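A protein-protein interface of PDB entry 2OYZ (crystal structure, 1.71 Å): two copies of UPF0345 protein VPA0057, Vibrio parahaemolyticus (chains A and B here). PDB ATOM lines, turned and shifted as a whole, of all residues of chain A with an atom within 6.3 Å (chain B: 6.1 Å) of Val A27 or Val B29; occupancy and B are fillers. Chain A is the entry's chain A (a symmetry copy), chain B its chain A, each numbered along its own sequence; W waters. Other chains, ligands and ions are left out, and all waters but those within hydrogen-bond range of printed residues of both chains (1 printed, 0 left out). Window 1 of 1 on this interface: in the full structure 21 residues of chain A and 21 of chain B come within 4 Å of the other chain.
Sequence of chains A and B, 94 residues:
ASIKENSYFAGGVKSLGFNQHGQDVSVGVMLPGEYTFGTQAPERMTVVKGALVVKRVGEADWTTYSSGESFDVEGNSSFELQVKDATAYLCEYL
NZ of Lys B14 is in hydrogen-bond range of O of Ile A3, at 2.7 Å.
Lys A14 touches Leu B16, and with the chains exchanged Leu A16 touches Lys B14.
Leu A16 touches Val B29, and with the chains exchanged Val A29 touches Leu B16.
Val A27 touches Val B29, and with the chains exchanged Val A29 touches Val B27.
Val A48 touches its own counterpart, Val B48.
Positions printed for both chains: 14, 15, 16, 27, 28, 29, 48 and 89.
Of the 16 pairs that touch across the chains among the printed residues, 7 have their exchanged pair printed and touching as well.
Among the printed residues, merely in contact across the chains: Val A27 with Ala B88 (3.4 Å), Lys A14 with Leu B16 (3.4 Å), Leu A16 with Lys B14 (3.4 Å), Phe A18 with Val B29 (3.5 Å), Val A27 with Val B29 (3.6 Å), Val A29 with Val B27 (3.6 Å), Ile A3 with Val B29 (3.6 Å), Ile A3 with Gly B11 (3.6 Å), Phe A18 with Ala B86 (3.6 Å), Val A48 with Val B48 (3.7 Å), Ile A3 with Leu B31 (3.7 Å), Phe A18 with Ala B88 (3.8 Å), Ile A3 with Gly B12 (3.8 Å), Leu A16 with Val B29 (3.96 Å) and Val A29 with Leu B16 (3.96 Å).
Of the 16 printed residues of chain B, 10 touch a printed residue of chain A.
Hydrophobic or aromatic side chains of chain B that line the printed part of chain A: Leu B16, Val B27, Val B29, Leu B31, Val B48, Ala B86 and Ala B88.
Along chain B the printed residues that touch a printed residue of chain A span positions 11 to 88.
Of the 15 printed residues of chain A, 7 touch a printed residue of chain B.
Hydrophobic or aromatic side chains of chain A that line the printed part of chain B: Ile A3, Leu A16, Phe A18, Val A27, Val A29 and Val A48.
Among the printed residues, 16 pairs touch across the chains.
O of Ala B88 is in hydrogen-bond range of N of Val B48 (2.9 Å).
The backbone carbonyl oxygen (O) of Val B27 sits at hydrogen-bond distance from the backbone NH (N) of Leu B16.
The backbone NH (N) of Phe A18 lies within hydrogen-bond range of the backbone carbonyl oxygen (O) of Val A25, 2.9 Å away.
The backbone NH of Val A29 lies within hydrogen-bond range of the backbone carbonyl oxygen of Lys A14, 2.9 Å away.
The backbone NH (N) of Leu A16 lies within hydrogen-bond range of the backbone carbonyl oxygen (O) of Val A27 (2.7 Å).
The backbone NH (N) of Val B29 sits at hydrogen-bond distance from the backbone carbonyl oxygen (O) of Lys B14 (2.9 Å).
Water W1 lies within hydrogen-bond range of O of Gly B11 and N of Ile A3.
Of the printed residues of chain B, Lys A14 touches Leu B16 (3.4 Å).
Printed residues of chain B within 4 Å of Val A27: Val B29 (3.6 Å) and Ala B88 (3.4 Å).
Printed residues of chain A within 4 Å of Leu B16: Lys A14 and Val A29.
Gly B28 touches none of the printed residues of chain A.
Printed residues of chain A within 4 Å of Val B29: Ile A3, Leu A16, Phe A18 and Val A27.
Of the printed residues of chain A, Ala B86 touches Phe A18 (3.6 Å).
The nearest printed residue of chain A that does not touch Val B29 is Gly A17 (5.6 Å).
The nearest printed residue of chain A that does not touch Gly B11 is Leu A16 (8.3 Å).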
ATOM      1  N   ILE A   3     -23.992  -4.615  13.465  1.00  0.00           N
ATOM      2  CA  ILE A   3     -23.213  -4.021  12.341  1.00  0.00           C
ATOM      3  C   ILE A   3     -21.711  -4.201  12.551  1.00  0.00           C
ATOM      4  O   ILE A   3     -21.086  -3.603  13.465  1.00  0.00           O
ATOM      5  CB  ILE A   3     -23.493  -2.519  12.140  1.00  0.00           C
ATOM      6  CG1 ILE A   3     -24.991  -2.230  12.020  1.00  0.00           C
ATOM      7  CG2 ILE A   3     -22.715  -1.985  10.917  1.00  0.00           C
ATOM      8  CD1 ILE A   3     -25.346  -0.735  12.199  1.00  0.00           C
ATOM      9  N   LYS A  14     -12.639   0.591   4.405  1.00  0.00           N
ATOM     10  CA  LYS A  14     -13.410   0.232   5.598  1.00  0.00           C
ATOM     11  C   LYS A  14     -14.809  -0.163   5.182  1.00  0.00           C
ATOM     12  O   LYS A  14     -15.334   0.379   4.217  1.00  0.00           O
ATOM     13  CB  LYS A  14     -13.479   1.407   6.565  1.00  0.00           C
ATOM     14  CG  LYS A  14     -12.094   1.840   7.087  1.00  0.00           C
ATOM     15  CD  LYS A  14     -12.283   2.978   8.066  1.00  0.00           C
ATOM     16  CE  LYS A  14     -10.933   3.535   8.439  1.00  0.00           C
ATOM     17  NZ  LYS A  14     -11.045   4.639   9.424  1.00  0.00           N
ATOM     18  N   SER A  15     -15.394  -1.083   5.942  1.00  0.00           N
ATOM     19  CA  SER A  15     -16.703  -1.657   5.613  1.00  0.00           C
ATOM     20  C   SER A  15     -17.571  -1.844   6.865  1.00  0.00           C
ATOM     21  O   SER A  15     -17.080  -1.882   8.020  1.00  0.00           O
ATOM     22  CB  SER A  15     -16.539  -3.015   4.872  1.00  0.00           C
ATOM     23  OG  SER A  15     -16.059  -4.024   5.756  1.00  0.00           O
ATOM     24  N   LEU A  16     -18.870  -1.916   6.601  1.00  0.00           N
ATOM     25  CA  LEU A  16     -19.904  -2.167   7.607  1.00  0.00           C
ATOM     26  C   LEU A  16     -20.740  -3.342   7.109  1.00  0.00           C
ATOM     27  O   LEU A  16     -21.350  -3.262   6.050  1.00  0.00           O
ATOM     28  CB  LEU A  16     -20.780  -0.920   7.809  1.00  0.00           C
ATOM     29  CG  LEU A  16     -20.068   0.324   8.366  1.00  0.00           C
ATOM     30  CD1 LEU A  16     -21.038   1.515   8.300  1.00  0.00           C
ATOM     31  CD2 LEU A  16     -19.561   0.139   9.813  1.00  0.00           C
ATOM     32  N   GLY A  17     -20.724  -4.449   7.845  1.00  0.00           N
ATOM     33  CA  GLY A  17     -21.439  -5.644   7.406  1.00  0.00           C
ATOM     34  C   GLY A  17     -22.714  -5.818   8.188  1.00  0.00           C
ATOM     35  O   GLY A  17     -22.802  -5.443   9.367  1.00  0.00           O
ATOM     36  N   PHE A  18     -23.712  -6.425   7.555  1.00  0.00           N
ATOM     37  CA  PHE A  18     -24.998  -6.550   8.199  1.00  0.00           C
ATOM     38  C   PHE A  18     -25.808  -7.608   7.481  1.00  0.00           C
ATOM     39  O   PHE A  18     -25.525  -7.932   6.338  1.00  0.00           O
ATOM     40  CB  PHE A  18     -25.732  -5.183   8.269  1.00  0.00           C
ATOM     41  CG  PHE A  18     -26.097  -4.603   6.932  1.00  0.00           C
ATOM     42  CD1 PHE A  18     -25.156  -3.889   6.181  1.00  0.00           C
ATOM     43  CD2 PHE A  18     -27.403  -4.737   6.428  1.00  0.00           C
ATOM     44  CE1 PHE A  18     -25.504  -3.340   4.952  1.00  0.00           C
ATOM     45  CE2 PHE A  18     -27.753  -4.172   5.187  1.00  0.00           C
ATOM     46  CZ  PHE A  18     -26.809  -3.489   4.458  1.00  0.00           C
ATOM     47  N   VAL A  25     -24.569  -8.647   3.686  1.00  0.00           N
ATOM     48  CA  VAL A  25     -24.310  -7.522   2.822  1.00  0.00           C
ATOM     49  C   VAL A  25     -23.251  -6.677   3.511  1.00  0.00           C
ATOM     50  O   VAL A  25     -23.108  -6.702   4.745  1.00  0.00           O
ATOM     51  CB  VAL A  25     -25.616  -6.665   2.663  1.00  0.00           C
ATOM     52  CG1 VAL A  25     -25.420  -5.562   1.655  1.00  0.00           C
ATOM     53  CG2 VAL A  25     -26.794  -7.518   2.244  1.00  0.00           C
ATOM     54  N   SER A  26     -22.485  -5.923   2.728  1.00  0.00           N
ATOM     55  CA  SER A  26     -21.630  -4.936   3.337  1.00  0.00           C
ATOM     56  C   SER A  26     -21.613  -3.667   2.481  1.00  0.00           C
ATOM     57  O   SER A  26     -21.792  -3.738   1.268  1.00  0.00           O
ATOM     58  CB  SER A  26     -20.219  -5.486   3.558  1.00  0.00           C
ATOM     59  OG  SER A  26     -19.585  -5.751   2.342  1.00  0.00           O
ATOM     60  N   VAL A  27     -21.522  -2.527   3.143  1.00  0.00           N
ATOM     61  CA  VAL A  27     -21.250  -1.268   2.461  1.00  0.00           C
ATOM     62  C   VAL A  27     -19.925  -0.750   2.950  1.00  0.00           C
ATOM     63  O   VAL A  27     -19.511  -1.034   4.084  1.00  0.00           O
ATOM     64  CB  VAL A  27     -22.347  -0.212   2.687  1.00  0.00           C
ATOM     65  CG1 VAL A  27     -23.590  -0.666   2.007  1.00  0.00           C
ATOM     66  CG2 VAL A  27     -22.618  -0.017   4.168  1.00  0.00           C
ATOM     67  N   GLY A  28     -19.219  -0.025   2.096  1.00  0.00           N
ATOM     68  CA  GLY A  28     -17.928   0.455   2.521  1.00  0.00           C
ATOM     69  C   GLY A  28     -17.429   1.581   1.660  1.00  0.00           C
ATOM     70  O   GLY A  28     -18.134   2.049   0.748  1.00  0.00           O
ATOM     71  N   VAL A  29     -16.224   2.020   1.990  1.00  0.00           N
ATOM     72  CA  VAL A  29     -15.535   3.127   1.351  1.00  0.00           C
ATOM     73  C   VAL A  29     -14.110   2.670   1.021  1.00  0.00           C
ATOM     74  O   VAL A  29     -13.473   1.949   1.794  1.00  0.00           O
ATOM     75  CB  VAL A  29     -15.519   4.375   2.231  1.00  0.00           C
ATOM     76  CG1 VAL A  29     -14.748   5.506   1.532  1.00  0.00           C
ATOM     77  CG2 VAL A  29     -16.996   4.824   2.464  1.00  0.00           C
ATOM     78  N   VAL A  48     -21.733   2.599  -5.240  1.00  0.00           N
ATOM     79  CA  VAL A  48     -22.789   3.468  -4.691  1.00  0.00           C
ATOM     80  C   VAL A  48     -22.583   4.935  -5.086  1.00  0.00           C
ATOM     81  O   VAL A  48     -23.501   5.587  -5.588  1.00  0.00           O
ATOM     82  CB  VAL A  48     -22.884   3.314  -3.160  1.00  0.00           C
ATOM     83  CG1 VAL A  48     -23.861   4.347  -2.547  1.00  0.00           C
ATOM     84  CG2 VAL A  48     -23.264   1.881  -2.823  1.00  0.00           C
ATOM     85  N   TYR A  89     -19.229   1.730  -1.930  1.00  0.00           N
ATOM     86  CA  TYR A  89     -19.637   0.556  -2.681  1.00  0.00           C
ATOM     87  C   TYR A  89     -20.560  -0.296  -1.800  1.00  0.00           C
ATOM     88  O   TYR A  89     -20.594  -0.134  -0.572  1.00  0.00           O
ATOM     89  CB  TYR A  89     -18.397  -0.269  -3.104  1.00  0.00           C
ATOM     90  CG  TYR A  89     -17.706  -0.940  -1.922  1.00  0.00           C
ATOM     91  CD1 TYR A  89     -16.724  -0.254  -1.179  1.00  0.00           C
ATOM     92  CD2 TYR A  89     -18.043  -2.260  -1.537  1.00  0.00           C
ATOM     93  CE1 TYR A  89     -16.108  -0.855  -0.105  1.00  0.00           C
ATOM     94  CE2 TYR A  89     -17.451  -2.861  -0.447  1.00  0.00           C
ATOM     95  CZ  TYR A  89     -16.466  -2.150   0.262  1.00  0.00           C
ATOM     96  OH  TYR A  89     -15.870  -2.733   1.347  1.00  0.00           O
ATOM     97  N   LEU A  90     -21.250  -1.234  -2.447  1.00  0.00           N
ATOM     98  CA  LEU A  90     -22.099  -2.231  -1.789  1.00  0.00           C
ATOM     99  C   LEU A  90     -21.626  -3.573  -2.302  1.00  0.00           C
ATOM    100  O   LEU A  90     -21.299  -3.699  -3.470  1.00  0.00           O
ATOM    101  CB  LEU A  90     -23.576  -2.030  -2.189  1.00  0.00           C
ATOM    102  CG  LEU A  90     -24.586  -3.043  -1.674  1.00  0.00           C
ATOM    103  CD1 LEU A  90     -24.829  -2.724  -0.221  1.00  0.00           C
ATOM    104  CD2 LEU A  90     -25.875  -2.845  -2.451  1.00  0.00           C
ATOM    105  N   CYS A  91     -21.545  -4.563  -1.410  1.00  0.00           N
ATOM    106  CA  CYS A  91     -21.110  -5.925  -1.778  1.00  0.00           C
ATOM    107  C   CYS A  91     -22.123  -6.936  -1.280  1.00  0.00           C
ATOM    108  O   CYS A  91     -22.497  -6.893  -0.109  1.00  0.00           O
ATOM    109  CB  CYS A  91     -19.748  -6.224  -1.157  1.00  0.00           C
ATOM    110  SG  CYS A  91     -19.063  -7.775  -1.774  1.00  0.00           S
ATOM    111  N   GLY B  11     -24.817   1.686  18.789  1.00  0.00           N
ATOM    112  CA  GLY B  11     -24.413   0.798  17.694  1.00  0.00           C
ATOM    113  C   GLY B  11     -25.539   0.509  16.706  1.00  0.00           C
ATOM    114  O   GLY B  11     -25.362  -0.272  15.768  1.00  0.00           O
ATOM    115  N   GLY B  12     -26.688   1.151  16.922  1.00  0.00           N
ATOM    116  CA  GLY B  12     -27.848   1.036  16.048  1.00  0.00           C
ATOM    117  C   GLY B  12     -27.653   1.644  14.676  1.00  0.00           C
ATOM    118  O   GLY B  12     -28.281   1.210  13.710  1.00  0.00           O
ATOM    119  N   VAL B  13     -26.798   2.661  14.610  1.00  0.00           N
ATOM    120  CA  VAL B  13     -26.467   3.338  13.350  1.00  0.00           C
ATOM    121  C   VAL B  13     -24.948   3.514  13.342  1.00  0.00           C
ATOM    122  O   VAL B  13     -24.352   3.976  14.315  1.00  0.00           O
ATOM    123  CB  VAL B  13     -27.183   4.698  13.232  1.00  0.00           C
ATOM    124  CG1 VAL B  13     -26.749   5.430  11.960  1.00  0.00           C
ATOM    125  CG2 VAL B  13     -28.719   4.498  13.271  1.00  0.00           C
ATOM    126  N   LYS B  14     -24.312   3.079  12.261  1.00  0.00           N
ATOM    127  CA  LYS B  14     -22.887   3.356  12.066  1.00  0.00           C
ATOM    128  C   LYS B  14     -22.674   3.899  10.672  1.00  0.00           C
ATOM    129  O   LYS B  14     -23.385   3.513   9.752  1.00  0.00           O
ATOM    130  CB  LYS B  14     -22.065   2.086  12.248  1.00  0.00           C
ATOM    131  CG  LYS B  14     -22.178   1.494  13.667  1.00  0.00           C
ATOM    132  CD  LYS B  14     -21.293   0.268  13.749  1.00  0.00           C
ATOM    133  CE  LYS B  14     -21.537  -0.428  15.063  1.00  0.00           C
ATOM    134  NZ  LYS B  14     -20.677  -1.627  15.220  1.00  0.00           N
ATOM    135  N   SER B  15     -21.677   4.768  10.542  1.00  0.00           N
ATOM    136  CA  SER B  15     -21.407   5.473   9.284  1.00  0.00           C
ATOM    137  C   SER B  15     -19.902   5.579   9.005  1.00  0.00           C
ATOM    138  O   SER B  15     -19.042   5.448   9.910  1.00  0.00           O
ATOM    139  CB  SER B  15     -22.047   6.890   9.298  1.00  0.00           C
ATOM    140  OG  SER B  15     -21.358   7.753  10.199  1.00  0.00           O
ATOM    141  N   LEU B  16     -19.615   5.778   7.723  1.00  0.00           N
ATOM    142  CA  LEU B  16     -18.263   5.989   7.203  1.00  0.00           C
ATOM    143  C   LEU B  16     -18.293   7.274   6.379  1.00  0.00           C
ATOM    144  O   LEU B  16     -19.020   7.361   5.399  1.00  0.00           O
ATOM    145  CB  LEU B  16     -17.821   4.797   6.340  1.00  0.00           C
ATOM    146  CG  LEU B  16     -17.691   3.447   7.066  1.00  0.00           C
ATOM    147  CD1 LEU B  16     -17.452   2.348   6.018  1.00  0.00           C
ATOM    148  CD2 LEU B  16     -16.561   3.426   8.117  1.00  0.00           C
ATOM    149  N   VAL B  27     -21.659   6.980   4.017  1.00  0.00           N
ATOM    150  CA  VAL B  27     -22.486   5.791   3.853  1.00  0.00           C
ATOM    151  C   VAL B  27     -22.611   5.121   5.194  1.00  0.00           C
ATOM    152  O   VAL B  27     -21.721   5.242   6.050  1.00  0.00           O
ATOM    153  CB  VAL B  27     -21.918   4.801   2.819  1.00  0.00           C
ATOM    154  CG1 VAL B  27     -22.005   5.421   1.470  1.00  0.00           C
ATOM    155  CG2 VAL B  27     -20.473   4.458   3.131  1.00  0.00           C
ATOM    156  N   GLY B  28     -23.729   4.449   5.420  1.00  0.00           N
ATOM    157  CA  GLY B  28     -23.896   3.828   6.710  1.00  0.00           C
ATOM    158  C   GLY B  28     -24.967   2.773   6.699  1.00  0.00           C
ATOM    159  O   GLY B  28     -25.551   2.467   5.643  1.00  0.00           O
ATOM    160  N   VAL B  29     -25.183   2.209   7.877  1.00  0.00           N
ATOM    161  CA  VAL B  29     -26.126   1.135   8.128  1.00  0.00           C
ATOM    162  C   VAL B  29     -26.966   1.519   9.352  1.00  0.00           C
ATOM    163  O   VAL B  29     -26.462   2.095  10.319  1.00  0.00           O
ATOM    164  CB  VAL B  29     -25.423  -0.204   8.345  1.00  0.00           C
ATOM    165  CG1 VAL B  29     -26.455  -1.301   8.645  1.00  0.00           C
ATOM    166  CG2 VAL B  29     -24.650  -0.564   7.037  1.00  0.00           C
ATOM    167  N   MET B  30     -28.251   1.206   9.263  1.00  0.00           N
ATOM    168  CA  MET B  30     -29.190   1.385  10.396  1.00  0.00           C
ATOM    169  C   MET B  30     -29.867   0.073  10.655  1.00  0.00           C
ATOM    170  O   MET B  30     -30.396  -0.526   9.754  1.00  0.00           O
ATOM    171  CB  MET B  30     -30.246   2.447  10.068  1.00  0.00           C
ATOM    172  CG  MET B  30     -29.648   3.780   9.685  1.00  0.00           C
ATOM    173  SD  MET B  30     -31.074   5.157   9.586  1.00  0.00           S
ATOM    174  CE  MET B  30     -30.011   6.641   8.845  1.00  0.00           C
ATOM    175  N   LEU B  31     -29.866  -0.341  11.913  1.00  0.00           N
ATOM    176  CA  LEU B  31     -30.564  -1.531  12.348  1.00  0.00           C
ATOM    177  C   LEU B  31     -32.027  -1.180  12.616  1.00  0.00           C
ATOM    178  O   LEU B  31     -32.389  -0.005  12.874  1.00  0.00           O
ATOM    179  CB  LEU B  31     -29.915  -2.071  13.633  1.00  0.00           C
ATOM    180  CG  LEU B  31     -28.478  -2.635  13.485  1.00  0.00           C
ATOM    181  CD1 LEU B  31     -27.995  -3.145  14.814  1.00  0.00           C
ATOM    182  CD2 LEU B  31     -28.376  -3.755  12.442  1.00  0.00           C
ATOM    183  N   VAL B  48     -29.611   2.880  -0.054  1.00  0.00           N
ATOM    184  CA  VAL B  48     -28.750   2.034  -0.902  1.00  0.00           C
ATOM    185  C   VAL B  48     -29.304   0.611  -1.037  1.00  0.00           C
ATOM    186  O   VAL B  48     -29.442   0.092  -2.146  1.00  0.00           O
ATOM    187  CB  VAL B  48     -27.304   2.019  -0.370  1.00  0.00           C
ATOM    188  CG1 VAL B  48     -26.429   0.998  -1.140  1.00  0.00           C
ATOM    189  CG2 VAL B  48     -26.736   3.428  -0.420  1.00  0.00           C
ATOM    190  N   ALA B  86     -32.584  -4.141   8.534  1.00  0.00           N
ATOM    191  CA  ALA B  86     -31.272  -3.451   8.493  1.00  0.00           C
ATOM    192  C   ALA B  86     -31.047  -2.893   7.096  1.00  0.00           C
ATOM    193  O   ALA B  86     -31.198  -3.605   6.115  1.00  0.00           O
ATOM    194  CB  ALA B  86     -30.136  -4.375   8.848  1.00  0.00           C
ATOM    195  N   THR B  87     -30.658  -1.621   7.026  1.00  0.00           N
ATOM    196  CA  THR B  87     -30.671  -0.891   5.742  1.00  0.00           C
ATOM    197  C   THR B  87     -29.402  -0.052   5.573  1.00  0.00           C
ATOM    198  O   THR B  87     -29.005   0.616   6.510  1.00  0.00           O
ATOM    199  CB  THR B  87     -31.981   0.008   5.629  1.00  0.00           C
ATOM    200  OG1 THR B  87     -33.155  -0.817   5.433  1.00  0.00           O
ATOM    201  CG2 THR B  87     -31.908   1.000   4.458  1.00  0.00           C
ATOM    202  N   ALA B  88     -28.831  -0.058   4.367  1.00  0.00           N
ATOM    203  CA  ALA B  88     -27.667   0.790   4.024  1.00  0.00           C
ATOM    204  C   ALA B  88     -28.189   2.055   3.357  1.00  0.00           C
ATOM    205  O   ALA B  88     -29.183   1.994   2.623  1.00  0.00           O
ATOM    206  CB  ALA B  88     -26.731   0.072   3.090  1.00  0.00           C
ATOM    207  N   TYR B  89     -27.531   3.172   3.630  1.00  0.00           N
ATOM    208  CA  TYR B  89     -27.963   4.452   3.097  1.00  0.00           C
ATOM    209  C   TYR B  89     -26.725   5.265   2.699  1.00  0.00           C
ATOM    210  O   TYR B  89     -25.603   4.965   3.131  1.00  0.00           O
ATOM    211  CB  TYR B  89     -28.786   5.224   4.158  1.00  0.00           C
ATOM    212  CG  TYR B  89     -27.935   5.702   5.329  1.00  0.00           C
ATOM    213  CD1 TYR B  89     -27.702   4.864   6.438  1.00  0.00           C
ATOM    214  CD2 TYR B  89     -27.348   6.991   5.324  1.00  0.00           C
ATOM    215  CE1 TYR B  89     -26.925   5.289   7.490  1.00  0.00           C
ATOM    216  CE2 TYR B  89     -26.547   7.416   6.361  1.00  0.00           C
ATOM    217  CZ  TYR B  89     -26.349   6.557   7.457  1.00  0.00           C
ATOM    218  OH  TYR B  89     -25.555   6.965   8.493  1.00  0.00           O
HETATM  219  O   HOH W   1     -24.341  -2.943  15.761  1.00  0.00           O
